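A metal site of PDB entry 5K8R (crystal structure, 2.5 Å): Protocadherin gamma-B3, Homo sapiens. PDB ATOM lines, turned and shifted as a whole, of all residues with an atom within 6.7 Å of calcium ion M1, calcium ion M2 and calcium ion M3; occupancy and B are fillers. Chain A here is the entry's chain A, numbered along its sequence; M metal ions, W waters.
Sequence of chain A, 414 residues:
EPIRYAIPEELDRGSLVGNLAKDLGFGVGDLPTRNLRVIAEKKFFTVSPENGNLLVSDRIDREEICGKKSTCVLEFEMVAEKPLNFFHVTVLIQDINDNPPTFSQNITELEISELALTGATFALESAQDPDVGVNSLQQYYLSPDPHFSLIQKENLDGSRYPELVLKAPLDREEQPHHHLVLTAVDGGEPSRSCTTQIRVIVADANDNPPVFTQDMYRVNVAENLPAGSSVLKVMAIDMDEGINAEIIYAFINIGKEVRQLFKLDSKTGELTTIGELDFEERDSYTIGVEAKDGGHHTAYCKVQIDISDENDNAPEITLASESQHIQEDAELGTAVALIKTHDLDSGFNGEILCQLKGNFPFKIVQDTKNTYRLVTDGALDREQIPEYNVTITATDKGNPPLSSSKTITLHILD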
ATOM      1  N   GLU A 223      17.241 -14.948  19.277  1.00  0.00           N
ATOM      2  CA  GLU A 223      17.723 -16.296  18.988  1.00  0.00           C
ATOM      3  C   GLU A 223      18.094 -16.458  17.518  1.00  0.00           C
ATOM      4  O   GLU A 223      18.939 -17.299  17.186  1.00  0.00           O
ATOM      5  CB  GLU A 223      16.681 -17.337  19.387  1.00  0.00           C
ATOM      6  CG  GLU A 223      15.313 -17.105  18.785  1.00  0.00           C
ATOM      7  CD  GLU A 223      14.356 -18.253  19.058  1.00  0.00           C
ATOM      8  OE1 GLU A 223      14.843 -19.382  19.287  1.00  0.00           O
ATOM      9  OE2 GLU A 223      13.129 -18.026  19.061  1.00  0.00           O
ATOM     10  N   LEU A 277      22.000 -19.697  18.176  1.00  0.00           N
ATOM     11  CA  LEU A 277      21.246 -19.563  19.411  1.00  0.00           C
ATOM     12  C   LEU A 277      19.842 -20.110  19.219  1.00  0.00           C
ATOM     13  O   LEU A 277      19.213 -19.905  18.174  1.00  0.00           O
ATOM     14  CB  LEU A 277      21.186 -18.106  19.852  1.00  0.00           C
ATOM     15  CG  LEU A 277      22.478 -17.403  20.304  1.00  0.00           C
ATOM     16  CD1 LEU A 277      23.353 -18.354  21.111  1.00  0.00           C
ATOM     17  CD2 LEU A 277      23.245 -16.845  19.112  1.00  0.00           C
ATOM     18  N   ASP A 278      19.341 -20.807  20.236  1.00  0.00           N
ATOM     19  CA  ASP A 278      18.000 -21.387  20.201  1.00  0.00           C
ATOM     20  C   ASP A 278      17.325 -21.114  21.537  1.00  0.00           C
ATOM     21  O   ASP A 278      17.704 -21.694  22.558  1.00  0.00           O
ATOM     22  CB  ASP A 278      18.051 -22.884  19.905  1.00  0.00           C
ATOM     23  CG  ASP A 278      16.678 -23.472  19.631  1.00  0.00           C
ATOM     24  OD1 ASP A 278      15.753 -22.695  19.292  1.00  0.00           O
ATOM     25  OD2 ASP A 278      16.518 -24.698  19.750  1.00  0.00           O
ATOM     26  N   PHE A 279      16.334 -20.217  21.521  1.00  0.00           N
ATOM     27  CA  PHE A 279      15.606 -19.892  22.751  1.00  0.00           C
ATOM     28  C   PHE A 279      14.908 -21.124  23.320  1.00  0.00           C
ATOM     29  O   PHE A 279      14.783 -21.250  24.546  1.00  0.00           O
ATOM     30  CB  PHE A 279      14.590 -18.790  22.476  1.00  0.00           C
ATOM     31  CG  PHE A 279      13.766 -18.400  23.672  1.00  0.00           C
ATOM     32  CD1 PHE A 279      14.235 -17.463  24.573  1.00  0.00           C
ATOM     33  CD2 PHE A 279      12.522 -18.975  23.888  1.00  0.00           C
ATOM     34  CE1 PHE A 279      13.477 -17.099  25.671  1.00  0.00           C
ATOM     35  CE2 PHE A 279      11.759 -18.620  24.986  1.00  0.00           C
ATOM     36  CZ  PHE A 279      12.242 -17.679  25.889  1.00  0.00           C
ATOM     37  N   GLU A 280      14.465 -22.041  22.463  1.00  0.00           N
ATOM     38  CA  GLU A 280      13.795 -23.243  22.932  1.00  0.00           C
ATOM     39  C   GLU A 280      14.730 -24.171  23.685  1.00  0.00           C
ATOM     40  O   GLU A 280      14.254 -24.998  24.475  1.00  0.00           O
ATOM     41  CB  GLU A 280      13.158 -23.986  21.759  1.00  0.00           C
ATOM     42  CG  GLU A 280      11.789 -23.466  21.351  1.00  0.00           C
ATOM     43  CD  GLU A 280      11.820 -22.045  20.843  1.00  0.00           C
ATOM     44  OE1 GLU A 280      12.731 -21.712  20.056  1.00  0.00           O
ATOM     45  OE2 GLU A 280      10.937 -21.251  21.234  1.00  0.00           O
ATOM     46  N   GLU A 281      16.041 -24.057  23.478  1.00  0.00           N
ATOM     47  CA  GLU A 281      16.998 -24.905  24.175  1.00  0.00           C
ATOM     48  C   GLU A 281      17.529 -24.252  25.442  1.00  0.00           C
ATOM     49  O   GLU A 281      17.559 -24.878  26.500  1.00  0.00           O
ATOM     50  CB  GLU A 281      18.151 -25.270  23.236  1.00  0.00           C
ATOM     51  CG  GLU A 281      19.147 -26.256  23.832  1.00  0.00           C
ATOM     52  CD  GLU A 281      18.536 -27.619  24.114  1.00  0.00           C
ATOM     53  OE1 GLU A 281      17.584 -28.010  23.391  1.00  0.00           O
ATOM     54  OE2 GLU A 281      18.984 -28.297  25.054  1.00  0.00           O
ATOM     55  N   SER A 308      16.150 -13.741  23.657  1.00  0.00           N
ATOM     56  CA  SER A 308      14.741 -13.425  23.549  1.00  0.00           C
ATOM     57  C   SER A 308      14.062 -14.326  22.528  1.00  0.00           C
ATOM     58  O   SER A 308      14.690 -14.788  21.561  1.00  0.00           O
ATOM     59  CB  SER A 308      14.539 -11.953  23.160  1.00  0.00           C
ATOM     60  OG  SER A 308      15.271 -11.638  21.987  1.00  0.00           O
ATOM     61  N   ASP A 309      12.774 -14.579  22.754  1.00  0.00           N
ATOM     62  CA  ASP A 309      12.035 -15.547  21.944  1.00  0.00           C
ATOM     63  C   ASP A 309      11.645 -14.952  20.593  1.00  0.00           C
ATOM     64  O   ASP A 309      11.239 -13.787  20.507  1.00  0.00           O
ATOM     65  CB  ASP A 309      10.788 -16.013  22.698  1.00  0.00           C
ATOM     66  CG  ASP A 309       9.996 -17.044  21.916  1.00  0.00           C
ATOM     67  OD1 ASP A 309      10.611 -17.862  21.207  1.00  0.00           O
ATOM     68  OD2 ASP A 309       8.743 -17.031  22.018  1.00  0.00           O
ATOM     69  N   GLU A 310      11.778 -15.768  19.548  1.00  0.00           N
ATOM     70  CA  GLU A 310      11.332 -15.416  18.213  1.00  0.00           C
ATOM     71  C   GLU A 310      10.352 -16.477  17.718  1.00  0.00           C
ATOM     72  O   GLU A 310      10.418 -17.644  18.114  1.00  0.00           O
ATOM     73  CB  GLU A 310      12.509 -15.314  17.229  1.00  0.00           C
ATOM     74  CG  GLU A 310      13.325 -14.038  17.379  1.00  0.00           C
ATOM     75  CD  GLU A 310      12.653 -12.845  16.734  1.00  0.00           C
ATOM     76  OE1 GLU A 310      12.253 -12.952  15.556  1.00  0.00           O
ATOM     77  OE2 GLU A 310      12.513 -11.799  17.398  1.00  0.00           O
ATOM     78  N   ASN A 311       9.432 -16.050  16.855  1.00  0.00           N
ATOM     79  CA  ASN A 311       8.382 -16.946  16.352  1.00  0.00           C
ATOM     80  C   ASN A 311       8.913 -17.722  15.145  1.00  0.00           C
ATOM     81  O   ASN A 311       8.567 -17.471  13.991  1.00  0.00           O
ATOM     82  CB  ASN A 311       7.133 -16.149  15.997  1.00  0.00           C
ATOM     83  CG  ASN A 311       5.940 -17.043  15.724  1.00  0.00           C
ATOM     84  OD1 ASN A 311       5.877 -18.184  16.188  1.00  0.00           O
ATOM     85  ND2 ASN A 311       4.975 -16.523  14.977  1.00  0.00           N
ATOM     86  N   ASP A 312       9.788 -18.689  15.444  1.00  0.00           N
ATOM     87  CA  ASP A 312      10.412 -19.515  14.422  1.00  0.00           C
ATOM     88  C   ASP A 312       9.984 -20.971  14.489  1.00  0.00           C
ATOM     89  O   ASP A 312      10.678 -21.855  13.994  1.00  0.00           O
ATOM     90  CB  ASP A 312      11.939 -19.416  14.517  1.00  0.00           C
ATOM     91  CG  ASP A 312      12.483 -20.007  15.812  1.00  0.00           C
ATOM     92  OD1 ASP A 312      11.758 -19.994  16.829  1.00  0.00           O
ATOM     93  OD2 ASP A 312      13.635 -20.478  15.800  1.00  0.00           O
ATOM     94  N   ASN A 313       8.827 -21.248  15.106  1.00  0.00           N
ATOM     95  CA  ASN A 313       8.275 -22.588  15.182  1.00  0.00           C
ATOM     96  C   ASN A 313       6.797 -22.534  14.834  1.00  0.00           C
ATOM     97  O   ASN A 313       6.031 -21.837  15.499  1.00  0.00           O
ATOM     98  CB  ASN A 313       8.474 -23.191  16.582  1.00  0.00           C
ATOM     99  CG  ASN A 313       9.909 -23.635  16.830  1.00  0.00           C
ATOM    100  OD1 ASN A 313      10.255 -24.792  16.580  1.00  0.00           O
ATOM    101  ND2 ASN A 313      10.724 -22.723  17.323  1.00  0.00           N
ATOM    102  N   ALA A 314       6.415 -23.268  13.795  1.00  0.00           N
ATOM    103  CA  ALA A 314       5.033 -23.291  13.349  1.00  0.00           C
ATOM    104  C   ALA A 314       4.182 -24.183  14.245  1.00  0.00           C
ATOM    105  O   ALA A 314       4.688 -25.159  14.819  1.00  0.00           O
ATOM    106  CB  ALA A 314       4.938 -23.777  11.905  1.00  0.00           C
ATOM    107  N   PRO A 315       2.898 -23.866  14.413  1.00  0.00           N
ATOM    108  CA  PRO A 315       2.026 -24.723  15.230  1.00  0.00           C
ATOM    109  C   PRO A 315       1.902 -26.114  14.629  1.00  0.00           C
ATOM    110  O   PRO A 315       1.984 -26.296  13.408  1.00  0.00           O
ATOM    111  CB  PRO A 315       0.680 -23.984  15.212  1.00  0.00           C
ATOM    112  CG  PRO A 315       1.031 -22.568  14.871  1.00  0.00           C
ATOM    113  CD  PRO A 315       2.203 -22.657  13.957  1.00  0.00           C
ATOM    114  N   ASP A 343       2.743 -25.723  20.216  1.00  0.00           N
ATOM    115  CA  ASP A 343       3.705 -24.798  19.631  1.00  0.00           C
ATOM    116  C   ASP A 343       4.891 -24.673  20.573  1.00  0.00           C
ATOM    117  O   ASP A 343       4.713 -24.461  21.775  1.00  0.00           O
ATOM    118  CB  ASP A 343       3.077 -23.431  19.374  1.00  0.00           C
ATOM    119  CG  ASP A 343       3.888 -22.575  18.413  1.00  0.00           C
ATOM    120  OD1 ASP A 343       3.307 -22.041  17.445  1.00  0.00           O
ATOM    121  OD2 ASP A 343       5.115 -22.445  18.618  1.00  0.00           O
ATOM    122  N   LEU A 344       6.098 -24.802  20.026  1.00  0.00           N
ATOM    123  CA  LEU A 344       7.299 -24.801  20.851  1.00  0.00           C
ATOM    124  C   LEU A 344       7.685 -23.420  21.355  1.00  0.00           C
ATOM    125  O   LEU A 344       8.474 -23.314  22.304  1.00  0.00           O
ATOM    126  CB  LEU A 344       8.471 -25.404  20.072  1.00  0.00           C
ATOM    127  CG  LEU A 344       8.308 -26.841  19.580  1.00  0.00           C
ATOM    128  CD1 LEU A 344       9.531 -27.289  18.794  1.00  0.00           C
ATOM    129  CD2 LEU A 344       8.040 -27.792  20.744  1.00  0.00           C
ATOM    130  N   ASP A 345       7.150 -22.360  20.758  1.00  0.00           N
ATOM    131  CA  ASP A 345       7.515 -21.003  21.139  1.00  0.00           C
ATOM    132  C   ASP A 345       6.801 -20.605  22.435  1.00  0.00           C
ATOM    133  O   ASP A 345       5.977 -21.343  22.973  1.00  0.00           O
ATOM    134  CB  ASP A 345       7.206 -20.027  20.007  1.00  0.00           C
ATOM    135  CG  ASP A 345       7.989 -20.325  18.754  1.00  0.00           C
ATOM    136  OD1 ASP A 345       9.132 -20.825  18.866  1.00  0.00           O
ATOM    137  OD2 ASP A 345       7.473 -20.070  17.641  1.00  0.00           O
ATOM    138  N   SER A 346       7.125 -19.419  22.938  1.00  0.00           N
ATOM    139  CA  SER A 346       6.581 -18.921  24.192  1.00  0.00           C
ATOM    140  C   SER A 346       5.748 -17.668  23.942  1.00  0.00           C
ATOM    141  O   SER A 346       5.818 -17.052  22.881  1.00  0.00           O
ATOM    142  CB  SER A 346       7.706 -18.613  25.186  1.00  0.00           C
ATOM    143  OG  SER A 346       8.544 -19.731  25.382  1.00  0.00           O
ATOM    144  N   PHE A 348       2.711 -15.144  23.158  1.00  0.00           N
ATOM    145  CA  PHE A 348       1.750 -15.155  22.069  1.00  0.00           C
ATOM    146  C   PHE A 348       2.291 -15.880  20.838  1.00  0.00           C
ATOM    147  O   PHE A 348       1.497 -16.292  19.982  1.00  0.00           O
ATOM    148  CB  PHE A 348       1.343 -13.729  21.700  1.00  0.00           C
ATOM    149  CG  PHE A 348       0.317 -13.137  22.638  1.00  0.00           C
ATOM    150  CD1 PHE A 348      -0.999 -13.548  22.600  1.00  0.00           C
ATOM    151  CD2 PHE A 348       0.684 -12.166  23.558  1.00  0.00           C
ATOM    152  CE1 PHE A 348      -1.945 -13.013  23.455  1.00  0.00           C
ATOM    153  CE2 PHE A 348      -0.251 -11.626  24.425  1.00  0.00           C
ATOM    154  CZ  PHE A 348      -1.568 -12.047  24.368  1.00  0.00           C
ATOM    155  N   ASN A 349       3.611 -16.045  20.732  1.00  0.00           N
ATOM    156  CA  ASN A 349       4.160 -16.887  19.689  1.00  0.00           C
ATOM    157  C   ASN A 349       3.764 -18.347  19.863  1.00  0.00           C
ATOM    158  O   ASN A 349       3.811 -19.115  18.901  1.00  0.00           O
ATOM    159  CB  ASN A 349       5.691 -16.768  19.660  1.00  0.00           C
ATOM    160  CG  ASN A 349       6.167 -15.340  19.522  1.00  0.00           C
ATOM    161  OD1 ASN A 349       5.542 -14.516  18.842  1.00  0.00           O
ATOM    162  ND2 ASN A 349       7.282 -15.017  20.177  1.00  0.00           N
ATOM    163  N   GLY A 350       3.366 -18.734  21.080  1.00  0.00           N
ATOM    164  CA  GLY A 350       2.966 -20.100  21.346  1.00  0.00           C
ATOM    165  C   GLY A 350       1.471 -20.284  21.469  1.00  0.00           C
ATOM    166  O   GLY A 350       0.983 -21.421  21.452  1.00  0.00           O
ATOM    167  N   GLU A 351       0.723 -19.190  21.587  1.00  0.00           N
ATOM    168  CA  GLU A 351      -0.725 -19.275  21.595  1.00  0.00           C
ATOM    169  C   GLU A 351      -1.223 -19.719  20.231  1.00  0.00           C
ATOM    170  O   GLU A 351      -0.697 -19.300  19.196  1.00  0.00           O
ATOM    171  CB  GLU A 351      -1.341 -17.921  21.973  1.00  0.00           C
ATOM    172  CG  GLU A 351      -0.891 -17.381  23.319  1.00  0.00           C
ATOM    173  CD  GLU A 351      -1.378 -18.222  24.485  1.00  0.00           C
ATOM    174  OE1 GLU A 351      -2.399 -18.925  24.334  1.00  0.00           O
ATOM    175  OE2 GLU A 351      -0.735 -18.182  25.558  1.00  0.00           O
ATOM    176  N   ASP A 396      -0.581 -19.469  14.921  1.00  0.00           N
ATOM    177  CA  ASP A 396      -0.171 -18.852  16.171  1.00  0.00           C
ATOM    178  C   ASP A 396      -0.452 -17.355  16.142  1.00  0.00           C
ATOM    179  O   ASP A 396      -0.922 -16.804  15.140  1.00  0.00           O
ATOM    180  CB  ASP A 396       1.303 -19.145  16.461  1.00  0.00           C
ATOM    181  CG  ASP A 396       2.216 -18.748  15.310  1.00  0.00           C
ATOM    182  OD1 ASP A 396       1.867 -17.850  14.526  1.00  0.00           O
ATOM    183  OD2 ASP A 396       3.310 -19.348  15.190  1.00  0.00           O
ATOM    184  N   LYS A 397      -0.166 -16.681  17.253  1.00  0.00           N
ATOM    185  CA  LYS A 397      -0.405 -15.252  17.391  1.00  0.00           C
ATOM    186  C   LYS A 397       0.892 -14.452  17.437  1.00  0.00           C
ATOM    187  O   LYS A 397       0.978 -13.419  18.100  1.00  0.00           O
ATOM    188  CB  LYS A 397      -1.235 -14.973  18.650  1.00  0.00           C
ATOM    189  CG  LYS A 397      -2.519 -15.802  18.732  1.00  0.00           C
ATOM    190  CD  LYS A 397      -3.356 -15.394  19.924  1.00  0.00           C
ATOM    191  CE  LYS A 397      -4.528 -16.352  20.120  1.00  0.00           C
ATOM    192  NZ  LYS A 397      -5.366 -16.468  18.899  1.00  0.00           N
ATOM    193  N   GLY A 398       1.918 -14.917  16.710  1.00  0.00           N
ATOM    194  CA  GLY A 398       3.187 -14.228  16.661  1.00  0.00           C
ATOM    195  C   GLY A 398       3.238 -13.178  15.562  1.00  0.00           C
ATOM    196  O   GLY A 398       2.286 -12.974  14.809  1.00  0.00           O
ATOM    197  N   LEU A 402       2.644 -17.686  12.113  1.00  0.00           N
ATOM    198  CA  LEU A 402       2.907 -18.915  11.387  1.00  0.00           C
ATOM    199  C   LEU A 402       1.722 -19.856  11.528  1.00  0.00           C
ATOM    200  O   LEU A 402       0.970 -19.783  12.504  1.00  0.00           O
ATOM    201  CB  LEU A 402       4.190 -19.615  11.880  1.00  0.00           C
ATOM    202  CG  LEU A 402       5.530 -19.108  11.331  1.00  0.00           C
ATOM    203  CD1 LEU A 402       5.887 -17.734  11.892  1.00  0.00           C
ATOM    204  CD2 LEU A 402       6.636 -20.101  11.631  1.00  0.00           C
HETATM  205 CA    CA M   1      14.038 -21.359  18.039  1.00  0.00          CA
HETATM  206 CA    CA M   2      11.216 -19.520  19.462  1.00  0.00          CA
HETATM  207 CA    CA M   3       5.000 -20.298  17.083  1.00  0.00          CA
HETATM  208  O   HOH W   1      13.201 -23.707  15.611  1.00  0.00           O
HETATM  209  O   HOH W   2      16.312 -21.812  17.033  1.00  0.00           O
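Within 4 Å of calcium ion M2: Glu 223, Glu 280, Asp 309, Glu 310, Asp 312, Asn 313 and Asp 345. The nearest printed residue that does not touch calcium ion M2 is Phe 279 (4.6 Å).
Calcium ion M1 is bound by OE1 of Glu 280 (2.4 Å), OD2 of Asp 312 (2.4 Å), OE1 of Glu 223 (2.5 Å), OD1 of Asp 278 (2.5 Å) and water W2 (2.5 Å). Calcium ion M1 has five donor atoms within binding distance. Slightly farther from calcium ion M1 lies OD1 of Asp 312 (2.9 Å).
O of Glu 310 binds calcium ion M2. The side-chain carboxylate (OE2) of Glu 223 is bound to calcium ion M2. Calcium ion M2 is bound by the side-chain carboxylate (OD1) of Asp 309 (2.5 Å). OE2 of Glu 280 binds calcium ion M2 (2.5 Å). OD1 of Asp 345 is bound to calcium ion M2. Calcium ion M2 is bound by OD1 of Asp 312 (2.7 Å). The side-chain carboxylate (OE1) of Glu 280 binds calcium ion M2, at 2.7 Å. Calcium ion M2 has seven donor atoms within binding distance.
OD1 of Asp 312 sits close to ND2 of Asn 313, 3.0 Å away. The side-chain carboxylate of Glu 223 sits close to the backbone NH of Phe 279, at 2.8 Å. The backbone carbonyl oxygen of Ser 308 sits at hydrogen-bond distance from the backbone NH of Glu 223 (3.4 Å). ND2 of Asn 349 is in hydrogen-bond range of OD2 of Asp 309, 3.1 Å away. OD2 of Asp 309 sits at hydrogen-bond distance from N of Ser 346 (3.0 Å). OD1 of Asp 396 sits at hydrogen-bond distance from N of Leu 402, at 2.5 Å.
O of Asn 313 is bound to calcium ion M3 (2.4 Å). The side-chain carboxylate (OD1) of Asp 343 is bound to calcium ion M3 (2.5 Å). Calcium ion M3 is bound by OD1 of Asn 311, at 2.5 Å. O of Asn 349 binds calcium ion M3. OD2 of Asp 345 is bound to calcium ion M3 (2.5 Å). OD2 of Asp 343 binds calcium ion M3 (2.6 Å). The side-chain carboxylate (OD2) of Asp 396 binds calcium ion M3, at 2.7 Å. Calcium ion M3 has seven donor atoms within binding distance.
Within 4 Å of calcium ion M1: Glu 223, Asp 278, Glu 280, Asp 312 and Asn 313.
Of the 26 residues printed, 6 come within 4 Å of calcium ion M3. The nearest printed residue that does not touch calcium ion M3 is Gly 350 (4.6 Å).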
